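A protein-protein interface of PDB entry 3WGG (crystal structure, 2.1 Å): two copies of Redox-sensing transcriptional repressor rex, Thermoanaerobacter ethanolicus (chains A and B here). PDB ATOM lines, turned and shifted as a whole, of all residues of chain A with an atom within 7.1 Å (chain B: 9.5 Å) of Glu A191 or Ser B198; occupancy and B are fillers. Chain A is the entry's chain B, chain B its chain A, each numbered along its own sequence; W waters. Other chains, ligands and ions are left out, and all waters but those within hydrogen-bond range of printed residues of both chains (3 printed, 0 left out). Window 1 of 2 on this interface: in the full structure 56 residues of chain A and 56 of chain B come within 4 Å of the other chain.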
ATOM      1  N   MET A   9     -13.135  -9.140  23.866  1.00  0.00           N
ATOM      2  CA  MET A   9     -12.667  -7.960  23.137  1.00  0.00           C
ATOM      3  C   MET A   9     -13.606  -6.735  23.268  1.00  0.00           C
ATOM      4  O   MET A   9     -13.160  -5.610  23.337  1.00  0.00           O
ATOM      5  CB  MET A   9     -12.457  -8.291  21.649  1.00  0.00           C
ATOM      6  CG  MET A   9     -11.152  -9.025  21.343  1.00  0.00           C
ATOM      7  SD  MET A   9      -9.745  -8.056  21.942  1.00  0.00           S
ATOM      8  CE  MET A   9      -9.672  -6.609  20.908  1.00  0.00           C
ATOM      9  N   ARG A  13     -11.973  -3.195  24.481  1.00  0.00           N
ATOM     10  CA  ARG A  13     -11.982  -1.956  23.672  1.00  0.00           C
ATOM     11  C   ARG A  13     -12.591  -0.746  24.351  1.00  0.00           C
ATOM     12  O   ARG A  13     -12.190   0.413  24.056  1.00  0.00           O
ATOM     13  CB  ARG A  13     -12.683  -2.171  22.315  1.00  0.00           C
ATOM     14  CG  ARG A  13     -11.872  -3.065  21.401  1.00  0.00           C
ATOM     15  CD  ARG A  13     -12.348  -2.935  19.940  1.00  0.00           C
ATOM     16  NE  ARG A  13     -11.667  -3.925  19.104  1.00  0.00           N
ATOM     17  CZ  ARG A  13     -10.431  -3.773  18.608  1.00  0.00           C
ATOM     18  NH1 ARG A  13      -9.685  -2.715  18.945  1.00  0.00           N
ATOM     19  NH2 ARG A  13      -9.890  -4.731  17.858  1.00  0.00           N
ATOM     20  N   PRO A  16      -9.583   1.492  27.013  1.00  0.00           N
ATOM     21  CA  PRO A  16      -8.766   2.679  26.751  1.00  0.00           C
ATOM     22  C   PRO A  16      -9.676   3.933  26.714  1.00  0.00           C
ATOM     23  O   PRO A  16      -9.204   5.013  26.961  1.00  0.00           O
ATOM     24  CB  PRO A  16      -8.164   2.419  25.356  1.00  0.00           C
ATOM     25  CG  PRO A  16      -8.302   0.901  25.090  1.00  0.00           C
ATOM     26  CD  PRO A  16      -9.599   0.535  25.888  1.00  0.00           C
ATOM     27  N   ALA A 173       3.271  -9.103  18.219  1.00  0.00           N
ATOM     28  CA  ALA A 173       2.028  -8.389  17.857  1.00  0.00           C
ATOM     29  C   ALA A 173       2.294  -7.545  16.646  1.00  0.00           C
ATOM     30  O   ALA A 173       3.405  -7.024  16.474  1.00  0.00           O
ATOM     31  CB  ALA A 173       1.545  -7.466  19.008  1.00  0.00           C
ATOM     32  N   ILE A 174       1.239  -7.316  15.886  1.00  0.00           N
ATOM     33  CA  ILE A 174       1.316  -6.478  14.684  1.00  0.00           C
ATOM     34  C   ILE A 174       0.196  -5.448  14.796  1.00  0.00           C
ATOM     35  O   ILE A 174      -0.972  -5.801  15.012  1.00  0.00           O
ATOM     36  CB  ILE A 174       1.171  -7.330  13.437  1.00  0.00           C
ATOM     37  CG1 ILE A 174       2.469  -8.159  13.276  1.00  0.00           C
ATOM     38  CG2 ILE A 174       0.886  -6.425  12.159  1.00  0.00           C
ATOM     39  CD1 ILE A 174       2.444  -9.083  12.024  1.00  0.00           C
ATOM     40  N   TRP A 175       0.589  -4.180  14.737  1.00  0.00           N
ATOM     41  CA  TRP A 175      -0.384  -3.065  14.700  1.00  0.00           C
ATOM     42  C   TRP A 175      -0.541  -2.711  13.212  1.00  0.00           C
ATOM     43  O   TRP A 175       0.399  -2.227  12.596  1.00  0.00           O
ATOM     44  CB  TRP A 175       0.151  -1.896  15.505  1.00  0.00           C
ATOM     45  CG  TRP A 175      -0.932  -0.916  15.888  1.00  0.00           C
ATOM     46  CD1 TRP A 175      -2.267  -1.188  16.046  1.00  0.00           C
ATOM     47  CD2 TRP A 175      -0.785   0.486  16.092  1.00  0.00           C
ATOM     48  NE1 TRP A 175      -2.945  -0.059  16.442  1.00  0.00           N
ATOM     49  CE2 TRP A 175      -2.081   1.009  16.392  1.00  0.00           C
ATOM     50  CE3 TRP A 175       0.306   1.363  16.054  1.00  0.00           C
ATOM     51  CZ2 TRP A 175      -2.279   2.340  16.765  1.00  0.00           C
ATOM     52  CZ3 TRP A 175       0.091   2.725  16.354  1.00  0.00           C
ATOM     53  CH2 TRP A 175      -1.183   3.192  16.707  1.00  0.00           C
ATOM     54  N   ASN A 176      -1.682  -3.049  12.606  1.00  0.00           N
ATOM     55  CA  ASN A 176      -1.791  -3.047  11.126  1.00  0.00           C
ATOM     56  C   ASN A 176      -2.683  -1.883  10.623  1.00  0.00           C
ATOM     57  O   ASN A 176      -3.869  -1.811  10.958  1.00  0.00           O
ATOM     58  CB  ASN A 176      -2.364  -4.402  10.626  1.00  0.00           C
ATOM     59  CG  ASN A 176      -2.713  -4.388   9.155  1.00  0.00           C
ATOM     60  OD1 ASN A 176      -1.957  -3.857   8.340  1.00  0.00           O
ATOM     61  ND2 ASN A 176      -3.875  -4.989   8.789  1.00  0.00           N
ATOM     62  N   PHE A 177      -2.115  -0.981   9.826  1.00  0.00           N
ATOM     63  CA  PHE A 177      -2.922   0.106   9.200  1.00  0.00           C
ATOM     64  C   PHE A 177      -3.571  -0.212   7.852  1.00  0.00           C
ATOM     65  O   PHE A 177      -4.331   0.610   7.328  1.00  0.00           O
ATOM     66  CB  PHE A 177      -2.067   1.356   9.054  1.00  0.00           C
ATOM     67  CG  PHE A 177      -1.876   2.077  10.347  1.00  0.00           C
ATOM     68  CD1 PHE A 177      -2.703   3.121  10.684  1.00  0.00           C
ATOM     69  CD2 PHE A 177      -0.976   1.602  11.288  1.00  0.00           C
ATOM     70  CE1 PHE A 177      -2.571   3.762  11.941  1.00  0.00           C
ATOM     71  CE2 PHE A 177      -0.782   2.289  12.493  1.00  0.00           C
ATOM     72  CZ  PHE A 177      -1.614   3.340  12.822  1.00  0.00           C
ATOM     73  N   VAL A 188      -0.137 -14.775  18.022  1.00  0.00           N
ATOM     74  CA  VAL A 188       0.322 -13.418  17.693  1.00  0.00           C
ATOM     75  C   VAL A 188      -0.889 -12.464  17.711  1.00  0.00           C
ATOM     76  O   VAL A 188      -1.957 -12.780  17.171  1.00  0.00           O
ATOM     77  CB  VAL A 188       1.014 -13.352  16.335  1.00  0.00           C
ATOM     78  CG1 VAL A 188       1.462 -11.863  16.008  1.00  0.00           C
ATOM     79  CG2 VAL A 188       2.299 -14.308  16.344  1.00  0.00           C
ATOM     80  N   ILE A 189      -0.744 -11.361  18.442  1.00  0.00           N
ATOM     81  CA  ILE A 189      -1.787 -10.372  18.514  1.00  0.00           C
ATOM     82  C   ILE A 189      -1.815  -9.573  17.210  1.00  0.00           C
ATOM     83  O   ILE A 189      -0.808  -9.000  16.787  1.00  0.00           O
ATOM     84  CB  ILE A 189      -1.585  -9.473  19.728  1.00  0.00           C
ATOM     85  CG1 ILE A 189      -1.858 -10.303  20.993  1.00  0.00           C
ATOM     86  CG2 ILE A 189      -2.595  -8.297  19.694  1.00  0.00           C
ATOM     87  CD1 ILE A 189      -1.075  -9.780  22.144  1.00  0.00           C
ATOM     88  N   LEU A 190      -2.971  -9.511  16.574  1.00  0.00           N
ATOM     89  CA  LEU A 190      -3.045  -8.680  15.406  1.00  0.00           C
ATOM     90  C   LEU A 190      -4.145  -7.619  15.630  1.00  0.00           C
ATOM     91  O   LEU A 190      -5.276  -7.967  15.957  1.00  0.00           O
ATOM     92  CB  LEU A 190      -3.306  -9.550  14.150  1.00  0.00           C
ATOM     93  CG  LEU A 190      -3.754  -8.755  12.921  1.00  0.00           C
ATOM     94  CD1 LEU A 190      -2.606  -7.903  12.290  1.00  0.00           C
ATOM     95  CD2 LEU A 190      -4.473  -9.613  11.898  1.00  0.00           C
ATOM     96  N   GLU A 191      -3.791  -6.347  15.563  1.00  0.00           N
ATOM     97  CA  GLU A 191      -4.791  -5.262  15.738  1.00  0.00           C
ATOM     98  C   GLU A 191      -4.873  -4.442  14.463  1.00  0.00           C
ATOM     99  O   GLU A 191      -3.875  -3.846  14.014  1.00  0.00           O
ATOM    100  CB  GLU A 191      -4.394  -4.362  16.927  1.00  0.00           C
ATOM    101  CG  GLU A 191      -5.129  -3.013  17.076  1.00  0.00           C
ATOM    102  CD  GLU A 191      -6.634  -3.189  17.408  1.00  0.00           C
ATOM    103  OE1 GLU A 191      -7.043  -4.350  17.603  1.00  0.00           O
ATOM    104  OE2 GLU A 191      -7.374  -2.174  17.510  1.00  0.00           O
ATOM    105  N   ASN A 192      -6.055  -4.403  13.871  1.00  0.00           N
ATOM    106  CA  ASN A 192      -6.209  -3.745  12.587  1.00  0.00           C
ATOM    107  C   ASN A 192      -6.785  -2.366  12.837  1.00  0.00           C
ATOM    108  O   ASN A 192      -7.845  -2.268  13.406  1.00  0.00           O
ATOM    109  CB  ASN A 192      -7.138  -4.590  11.649  1.00  0.00           C
ATOM    110  CG  ASN A 192      -6.552  -5.978  11.342  1.00  0.00           C
ATOM    111  OD1 ASN A 192      -5.403  -6.090  10.893  1.00  0.00           O
ATOM    112  ND2 ASN A 192      -7.299  -7.033  11.656  1.00  0.00           N
ATOM    113  N   VAL A 193      -6.100  -1.313  12.391  1.00  0.00           N
ATOM    114  CA  VAL A 193      -6.663   0.023  12.359  1.00  0.00           C
ATOM    115  C   VAL A 193      -7.460   0.218  11.048  1.00  0.00           C
ATOM    116  O   VAL A 193      -6.910   0.090   9.936  1.00  0.00           O
ATOM    117  CB  VAL A 193      -5.543   1.086  12.412  1.00  0.00           C
ATOM    118  CG1 VAL A 193      -6.122   2.527  12.347  1.00  0.00           C
ATOM    119  CG2 VAL A 193      -4.760   0.922  13.729  1.00  0.00           C
ATOM    120  N   HIS A 194      -8.746   0.500  11.167  1.00  0.00           N
ATOM    121  CA  HIS A 194      -9.551   0.821  10.009  1.00  0.00           C
ATOM    122  C   HIS A 194     -10.074   2.223  10.262  1.00  0.00           C
ATOM    123  O   HIS A 194     -11.112   2.390  10.922  1.00  0.00           O
ATOM    124  CB  HIS A 194     -10.732  -0.160   9.901  1.00  0.00           C
ATOM    125  CG  HIS A 194     -10.302  -1.564   9.591  1.00  0.00           C
ATOM    126  ND1 HIS A 194      -9.731  -1.915   8.384  1.00  0.00           N
ATOM    127  CD2 HIS A 194     -10.228  -2.663  10.374  1.00  0.00           C
ATOM    128  CE1 HIS A 194      -9.403  -3.198   8.412  1.00  0.00           C
ATOM    129  NE2 HIS A 194      -9.686  -3.671   9.615  1.00  0.00           N
ATOM    130  N   ARG B  17     -18.204  -1.627  10.787  1.00  0.00           N
ATOM    131  CA  ARG B  17     -17.505  -2.917  10.830  1.00  0.00           C
ATOM    132  C   ARG B  17     -18.364  -3.948  10.104  1.00  0.00           C
ATOM    133  O   ARG B  17     -17.875  -4.715   9.252  1.00  0.00           O
ATOM    134  CB  ARG B  17     -17.197  -3.362  12.256  1.00  0.00           C
ATOM    135  CG  ARG B  17     -16.343  -4.639  12.325  1.00  0.00           C
ATOM    136  CD  ARG B  17     -15.650  -4.752  13.721  1.00  0.00           C
ATOM    137  NE  ARG B  17     -14.734  -5.894  13.736  1.00  0.00           N
ATOM    138  CZ  ARG B  17     -14.976  -7.037  14.367  1.00  0.00           C
ATOM    139  NH1 ARG B  17     -16.067  -7.183  15.106  1.00  0.00           N
ATOM    140  NH2 ARG B  17     -14.116  -8.031  14.262  1.00  0.00           N
ATOM    141  N   ARG B  20     -17.783  -3.530   6.459  1.00  0.00           N
ATOM    142  CA  ARG B  20     -16.503  -4.114   5.982  1.00  0.00           C
ATOM    143  C   ARG B  20     -16.540  -5.619   5.763  1.00  0.00           C
ATOM    144  O   ARG B  20     -16.032  -6.130   4.765  1.00  0.00           O
ATOM    145  CB  ARG B  20     -15.332  -3.823   6.975  1.00  0.00           C
ATOM    146  CG  ARG B  20     -14.662  -2.526   6.749  1.00  0.00           C
ATOM    147  CD  ARG B  20     -13.402  -2.379   7.603  1.00  0.00           C
ATOM    148  NE  ARG B  20     -13.645  -2.221   9.051  1.00  0.00           N
ATOM    149  CZ  ARG B  20     -13.350  -3.171   9.916  1.00  0.00           C
ATOM    150  NH1 ARG B  20     -12.931  -4.367   9.442  1.00  0.00           N
ATOM    151  NH2 ARG B  20     -13.547  -2.980  11.208  1.00  0.00           N
ATOM    152  N   VAL B 193     -10.413  11.098  16.256  1.00  0.00           N
ATOM    153  CA  VAL B 193      -9.746   9.811  16.057  1.00  0.00           C
ATOM    154  C   VAL B 193      -8.793   9.683  17.246  1.00  0.00           C
ATOM    155  O   VAL B 193      -8.081  10.639  17.592  1.00  0.00           O
ATOM    156  CB  VAL B 193      -8.920   9.814  14.727  1.00  0.00           C
ATOM    157  CG1 VAL B 193      -8.106   8.497  14.549  1.00  0.00           C
ATOM    158  CG2 VAL B 193      -9.843  10.089  13.543  1.00  0.00           C
ATOM    159  N   HIS B 194      -8.772   8.515  17.867  1.00  0.00           N
ATOM    160  CA  HIS B 194      -7.842   8.287  18.955  1.00  0.00           C
ATOM    161  C   HIS B 194      -7.137   6.975  18.678  1.00  0.00           C
ATOM    162  O   HIS B 194      -7.639   5.938  19.110  1.00  0.00           O
ATOM    163  CB  HIS B 194      -8.660   8.147  20.248  1.00  0.00           C
ATOM    164  CG  HIS B 194      -9.333   9.419  20.650  1.00  0.00           C
ATOM    165  ND1 HIS B 194      -8.616  10.536  21.018  1.00  0.00           N
ATOM    166  CD2 HIS B 194     -10.641   9.776  20.686  1.00  0.00           C
ATOM    167  CE1 HIS B 194      -9.452  11.523  21.289  1.00  0.00           C
ATOM    168  NE2 HIS B 194     -10.686  11.085  21.114  1.00  0.00           N
ATOM    169  N   LEU B 195      -5.955   7.024  18.069  1.00  0.00           N
ATOM    170  CA  LEU B 195      -5.242   5.806  17.713  1.00  0.00           C
ATOM    171  C   LEU B 195      -4.796   5.063  18.967  1.00  0.00           C
ATOM    172  O   LEU B 195      -4.648   3.861  18.922  1.00  0.00           O
ATOM    173  CB  LEU B 195      -4.007   6.122  16.845  1.00  0.00           C
ATOM    174  CG  LEU B 195      -4.318   6.810  15.496  1.00  0.00           C
ATOM    175  CD1 LEU B 195      -2.969   7.030  14.684  1.00  0.00           C
ATOM    176  CD2 LEU B 195      -5.313   5.890  14.737  1.00  0.00           C
ATOM    177  N   SER B 196      -4.600   5.761  20.080  1.00  0.00           N
ATOM    178  CA  SER B 196      -4.208   5.087  21.341  1.00  0.00           C
ATOM    179  C   SER B 196      -5.324   4.146  21.800  1.00  0.00           C
ATOM    180  O   SER B 196      -5.004   3.142  22.416  1.00  0.00           O
ATOM    181  CB  SER B 196      -3.882   6.070  22.496  1.00  0.00           C
ATOM    182  OG  SER B 196      -5.079   6.796  22.793  1.00  0.00           O
ATOM    183  N   ASP B 197      -6.580   4.411  21.455  1.00  0.00           N
ATOM    184  CA  ASP B 197      -7.673   3.487  21.824  1.00  0.00           C
ATOM    185  C   ASP B 197      -7.429   2.115  21.166  1.00  0.00           C
ATOM    186  O   ASP B 197      -7.860   1.097  21.713  1.00  0.00           O
ATOM    187  CB  ASP B 197      -9.055   3.907  21.332  1.00  0.00           C
ATOM    188  CG  ASP B 197      -9.664   5.064  22.144  1.00  0.00           C
ATOM    189  OD1 ASP B 197      -9.021   5.525  23.082  1.00  0.00           O
ATOM    190  OD2 ASP B 197     -10.783   5.503  21.782  1.00  0.00           O
ATOM    191  N   SER B 198      -6.815   2.113  19.981  1.00  0.00           N
ATOM    192  CA  SER B 198      -6.411   0.845  19.333  1.00  0.00           C
ATOM    193  C   SER B 198      -5.086   0.355  19.902  1.00  0.00           C
ATOM    194  O   SER B 198      -4.970  -0.784  20.248  1.00  0.00           O
ATOM    195  CB  SER B 198      -6.280   1.020  17.802  1.00  0.00           C
ATOM    196  OG  SER B 198      -5.753  -0.132  17.142  1.00  0.00           O
ATOM    197  N   LEU B 199      -4.062   1.197  19.961  1.00  0.00           N
ATOM    198  CA  LEU B 199      -2.763   0.663  20.347  1.00  0.00           C
ATOM    199  C   LEU B 199      -2.817   0.068  21.751  1.00  0.00           C
ATOM    200  O   LEU B 199      -2.165  -0.930  22.013  1.00  0.00           O
ATOM    201  CB  LEU B 199      -1.714   1.729  20.342  1.00  0.00           C
ATOM    202  CG  LEU B 199      -0.302   1.340  20.755  1.00  0.00           C
ATOM    203  CD1 LEU B 199       0.348   0.323  19.854  1.00  0.00           C
ATOM    204  CD2 LEU B 199       0.575   2.599  20.801  1.00  0.00           C
ATOM    205  N   PHE B 200      -3.568   0.697  22.638  1.00  0.00           N
ATOM    206  CA  PHE B 200      -3.556   0.284  24.054  1.00  0.00           C
ATOM    207  C   PHE B 200      -4.286  -1.076  24.232  1.00  0.00           C
ATOM    208  O   PHE B 200      -4.119  -1.726  25.263  1.00  0.00           O
ATOM    209  CB  PHE B 200      -4.224   1.363  24.924  1.00  0.00           C
ATOM    210  CG  PHE B 200      -3.430   2.614  25.064  1.00  0.00           C
ATOM    211  CD1 PHE B 200      -2.145   2.697  24.588  1.00  0.00           C
ATOM    212  CD2 PHE B 200      -3.947   3.698  25.778  1.00  0.00           C
ATOM    213  CE1 PHE B 200      -1.381   3.888  24.757  1.00  0.00           C
ATOM    214  CE2 PHE B 200      -3.178   4.848  25.994  1.00  0.00           C
ATOM    215  CZ  PHE B 200      -1.905   4.953  25.462  1.00  0.00           C
ATOM    216  N   THR B 201      -5.040  -1.535  23.229  1.00  0.00           N
ATOM    217  CA  THR B 201      -5.580  -2.894  23.344  1.00  0.00           C
ATOM    218  C   THR B 201      -4.465  -3.914  23.070  1.00  0.00           C
ATOM    219  O   THR B 201      -4.593  -5.066  23.458  1.00  0.00           O
ATOM    220  CB  THR B 201      -6.757  -3.153  22.391  1.00  0.00           C
ATOM    221  OG1 THR B 201      -6.252  -3.176  21.051  1.00  0.00           O
ATOM    222  CG2 THR B 201      -7.804  -2.021  22.510  1.00  0.00           C
ATOM    223  N   VAL B 202      -3.371  -3.468  22.424  1.00  0.00           N
ATOM    224  CA  VAL B 202      -2.209  -4.329  22.138  1.00  0.00           C
ATOM    225  C   VAL B 202      -1.405  -4.549  23.405  1.00  0.00           C
ATOM    226  O   VAL B 202      -1.116  -5.677  23.736  1.00  0.00           O
ATOM    227  CB  VAL B 202      -1.306  -3.761  20.947  1.00  0.00           C
ATOM    228  CG1 VAL B 202      -0.157  -4.693  20.599  1.00  0.00           C
ATOM    229  CG2 VAL B 202      -2.167  -3.524  19.688  1.00  0.00           C
ATOM    230  N   SER B 203      -1.077  -3.471  24.131  1.00  0.00           N
ATOM    231  CA  SER B 203      -0.426  -3.607  25.423  1.00  0.00           C
ATOM    232  C   SER B 203      -1.344  -4.367  26.393  1.00  0.00           C
ATOM    233  O   SER B 203      -0.861  -5.183  27.156  1.00  0.00           O
ATOM    234  CB  SER B 203      -0.069  -2.241  26.014  1.00  0.00           C
ATOM    235  OG  SER B 203      -1.172  -1.369  25.814  1.00  0.00           O
ATOM    236  N   TYR B 204      -2.656  -4.162  26.302  1.00  0.00           N
ATOM    237  CA  TYR B 204      -3.563  -4.906  27.206  1.00  0.00           C
ATOM    238  C   TYR B 204      -3.376  -6.418  27.013  1.00  0.00           C
ATOM    239  O   TYR B 204      -3.120  -7.196  27.985  1.00  0.00           O
ATOM    240  CB  TYR B 204      -5.048  -4.478  27.021  1.00  0.00           C
ATOM    241  CG  TYR B 204      -5.943  -5.400  27.828  1.00  0.00           C
ATOM    242  CD1 TYR B 204      -6.280  -6.660  27.331  1.00  0.00           C
ATOM    243  CD2 TYR B 204      -6.274  -5.105  29.163  1.00  0.00           C
ATOM    244  CE1 TYR B 204      -7.009  -7.564  28.071  1.00  0.00           C
ATOM    245  CE2 TYR B 204      -6.991  -6.041  29.960  1.00  0.00           C
ATOM    246  CZ  TYR B 204      -7.394  -7.241  29.385  1.00  0.00           C
ATOM    247  OH  TYR B 204      -8.102  -8.164  30.110  1.00  0.00           O
ATOM    248  N   ARG B 205      -3.559  -6.843  25.767  1.00  0.00           N
ATOM    249  CA  ARG B 205      -3.466  -8.247  25.363  1.00  0.00           C
ATOM    250  C   ARG B 205      -2.099  -8.821  25.576  1.00  0.00           C
ATOM    251  O   ARG B 205      -2.008  -9.965  25.995  1.00  0.00           O
ATOM    252  CB  ARG B 205      -3.880  -8.427  23.889  1.00  0.00           C
ATOM    253  CG  ARG B 205      -5.395  -8.353  23.724  1.00  0.00           C
ATOM    254  CD  ARG B 205      -5.815  -8.484  22.265  1.00  0.00           C
ATOM    255  NE  ARG B 205      -5.740  -7.182  21.564  1.00  0.00           N
ATOM    256  CZ  ARG B 205      -6.100  -6.997  20.278  1.00  0.00           C
ATOM    257  NH1 ARG B 205      -6.523  -8.023  19.546  1.00  0.00           N
ATOM    258  NH2 ARG B 205      -6.082  -5.795  19.750  1.00  0.00           N
HETATM  259  O   HOH W   1     -10.110  -0.182  20.525  1.00  0.00           O
HETATM  260  O   HOH W   2      -6.564   5.579  24.803  1.00  0.00           O
HETATM  261  O   HOH W   3      -7.806  -7.558  17.143  1.00  0.00           O
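Of the printed residues of chain B, Glu A191 touches Ser B198, Thr B201, Val B202 and Arg B205. Ser B198 touches three residues of chain A. Leu A190 touches just one residue of chain B: Arg B205. No residue of chain B comes within 4 Å of Asn A192. Of the printed residues of chain B, Met A9 touches Arg B205 (3.6 Å). Printed residues of chain A within 4 Å of Arg B205: Met A9 (3.6 Å), Ile A189 (3.6 Å), Leu A190 (3.8 Å) and Glu A191 (2.8 Å). Printed residues of chain B within 4 Å of Ala A173: Val B202 (3.6 Å). Of the printed residues of chain A, Thr B201 touches Pro A16 (3.9 Å) and Glu A191 (3.7 Å). The nearest residue of chain B that does not touch Glu A191 is Leu B199 (5.2 Å). The nearest residue of chain A that does not touch Ser B198 is Asn A192 (4.8 Å).
The side-chain hydroxyl of Thr B201 lies within hydrogen-bond range of the guanidinium group of Arg B205 (2.9 Å). The backbone NH (N) of Ile A174 sits at hydrogen-bond distance from the backbone carbonyl oxygen (O) of Ile A189. O of Ser B198 sits at hydrogen-bond distance from OG1 of Thr B201 (2.8 Å). N of Asn A176 lies within hydrogen-bond range of O of Glu A191. The backbone carbonyl oxygen (O) of Ile A174 is in hydrogen-bond range of the backbone NH (N) of Glu A191, at 2.9 Å. The guanidinium group (NH1) of Arg A13 lies within salt-bridge range of the side-chain carboxylate (OE2) of Glu A191 (2.8 Å).
CE of Met A9 touches CZ of Arg B205 (3.6 Å). Pro A16 touches Asp B197. Thr B201 touches Pro A16 (CG2 to CG, 3.9 Å). Val B202 touches Ala A173. Leu B199 touches Trp A175. Ile A189 touches Arg B205. O of Leu A190 touches NH1 of Arg B205, 3.8 Å away. Thr B201 touches Glu A191 (OG1 to CD, 3.7 Å). CB of Glu A191 touches CG2 of Val B202 (3.6 Å). Ser B198 touches Val A193.
Positions printed for both chains: 193 and 194. Of the 15 pairs that touch across the chains among the printed residues, none has its exchanged pair printed and touching as well.
Of the 15 printed residues of chain A, 9 touch a printed residue of chain B. Hydrophobic or aromatic side chains of chain A that line the printed part of chain B: Met A9, Pro A16, Ala A173, Trp A175, Ile A189, Val A193 and His A194. Of the 15 printed residues of chain B, 8 touch a printed residue of chain A. Hydrophobic or aromatic side chains of chain B within 4 Å of the printed part of chain A: Leu B199 and Val B202.
Water W3 lies within hydrogen-bond range of the guanidinium group (NH1) of Arg B205, the backbone carbonyl oxygen (O) of Leu A190 and the side-chain carboxylate (OE1) of Glu A191. Water W2 lies within hydrogen-bond range of the side-chain hydroxyl of Ser B196, the side-chain carboxylate of Asp B197 and the backbone carbonyl oxygen of Pro A16. Water W1 lies within hydrogen-bond range of the backbone carbonyl oxygen (O) of Asp B197 (2.8 Å) and the guanidinium group (NH1) of Arg A13 (3.0 Å).
The side-chain hydroxyl (OG) of Ser B198 sits at hydrogen-bond distance from the indole nitrogen (NE1) of Trp A175 (2.9 Å). NH1 of Arg B20 sits at hydrogen-bond distance from NE2 of His A194, 3.3 Å away. OE2 of Glu A191 sits at hydrogen-bond distance from OG of Ser B198 (2.6 Å). NH2 of Arg B205 lies within salt-bridge range of OE1 of Glu A191 (2.8 Å).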
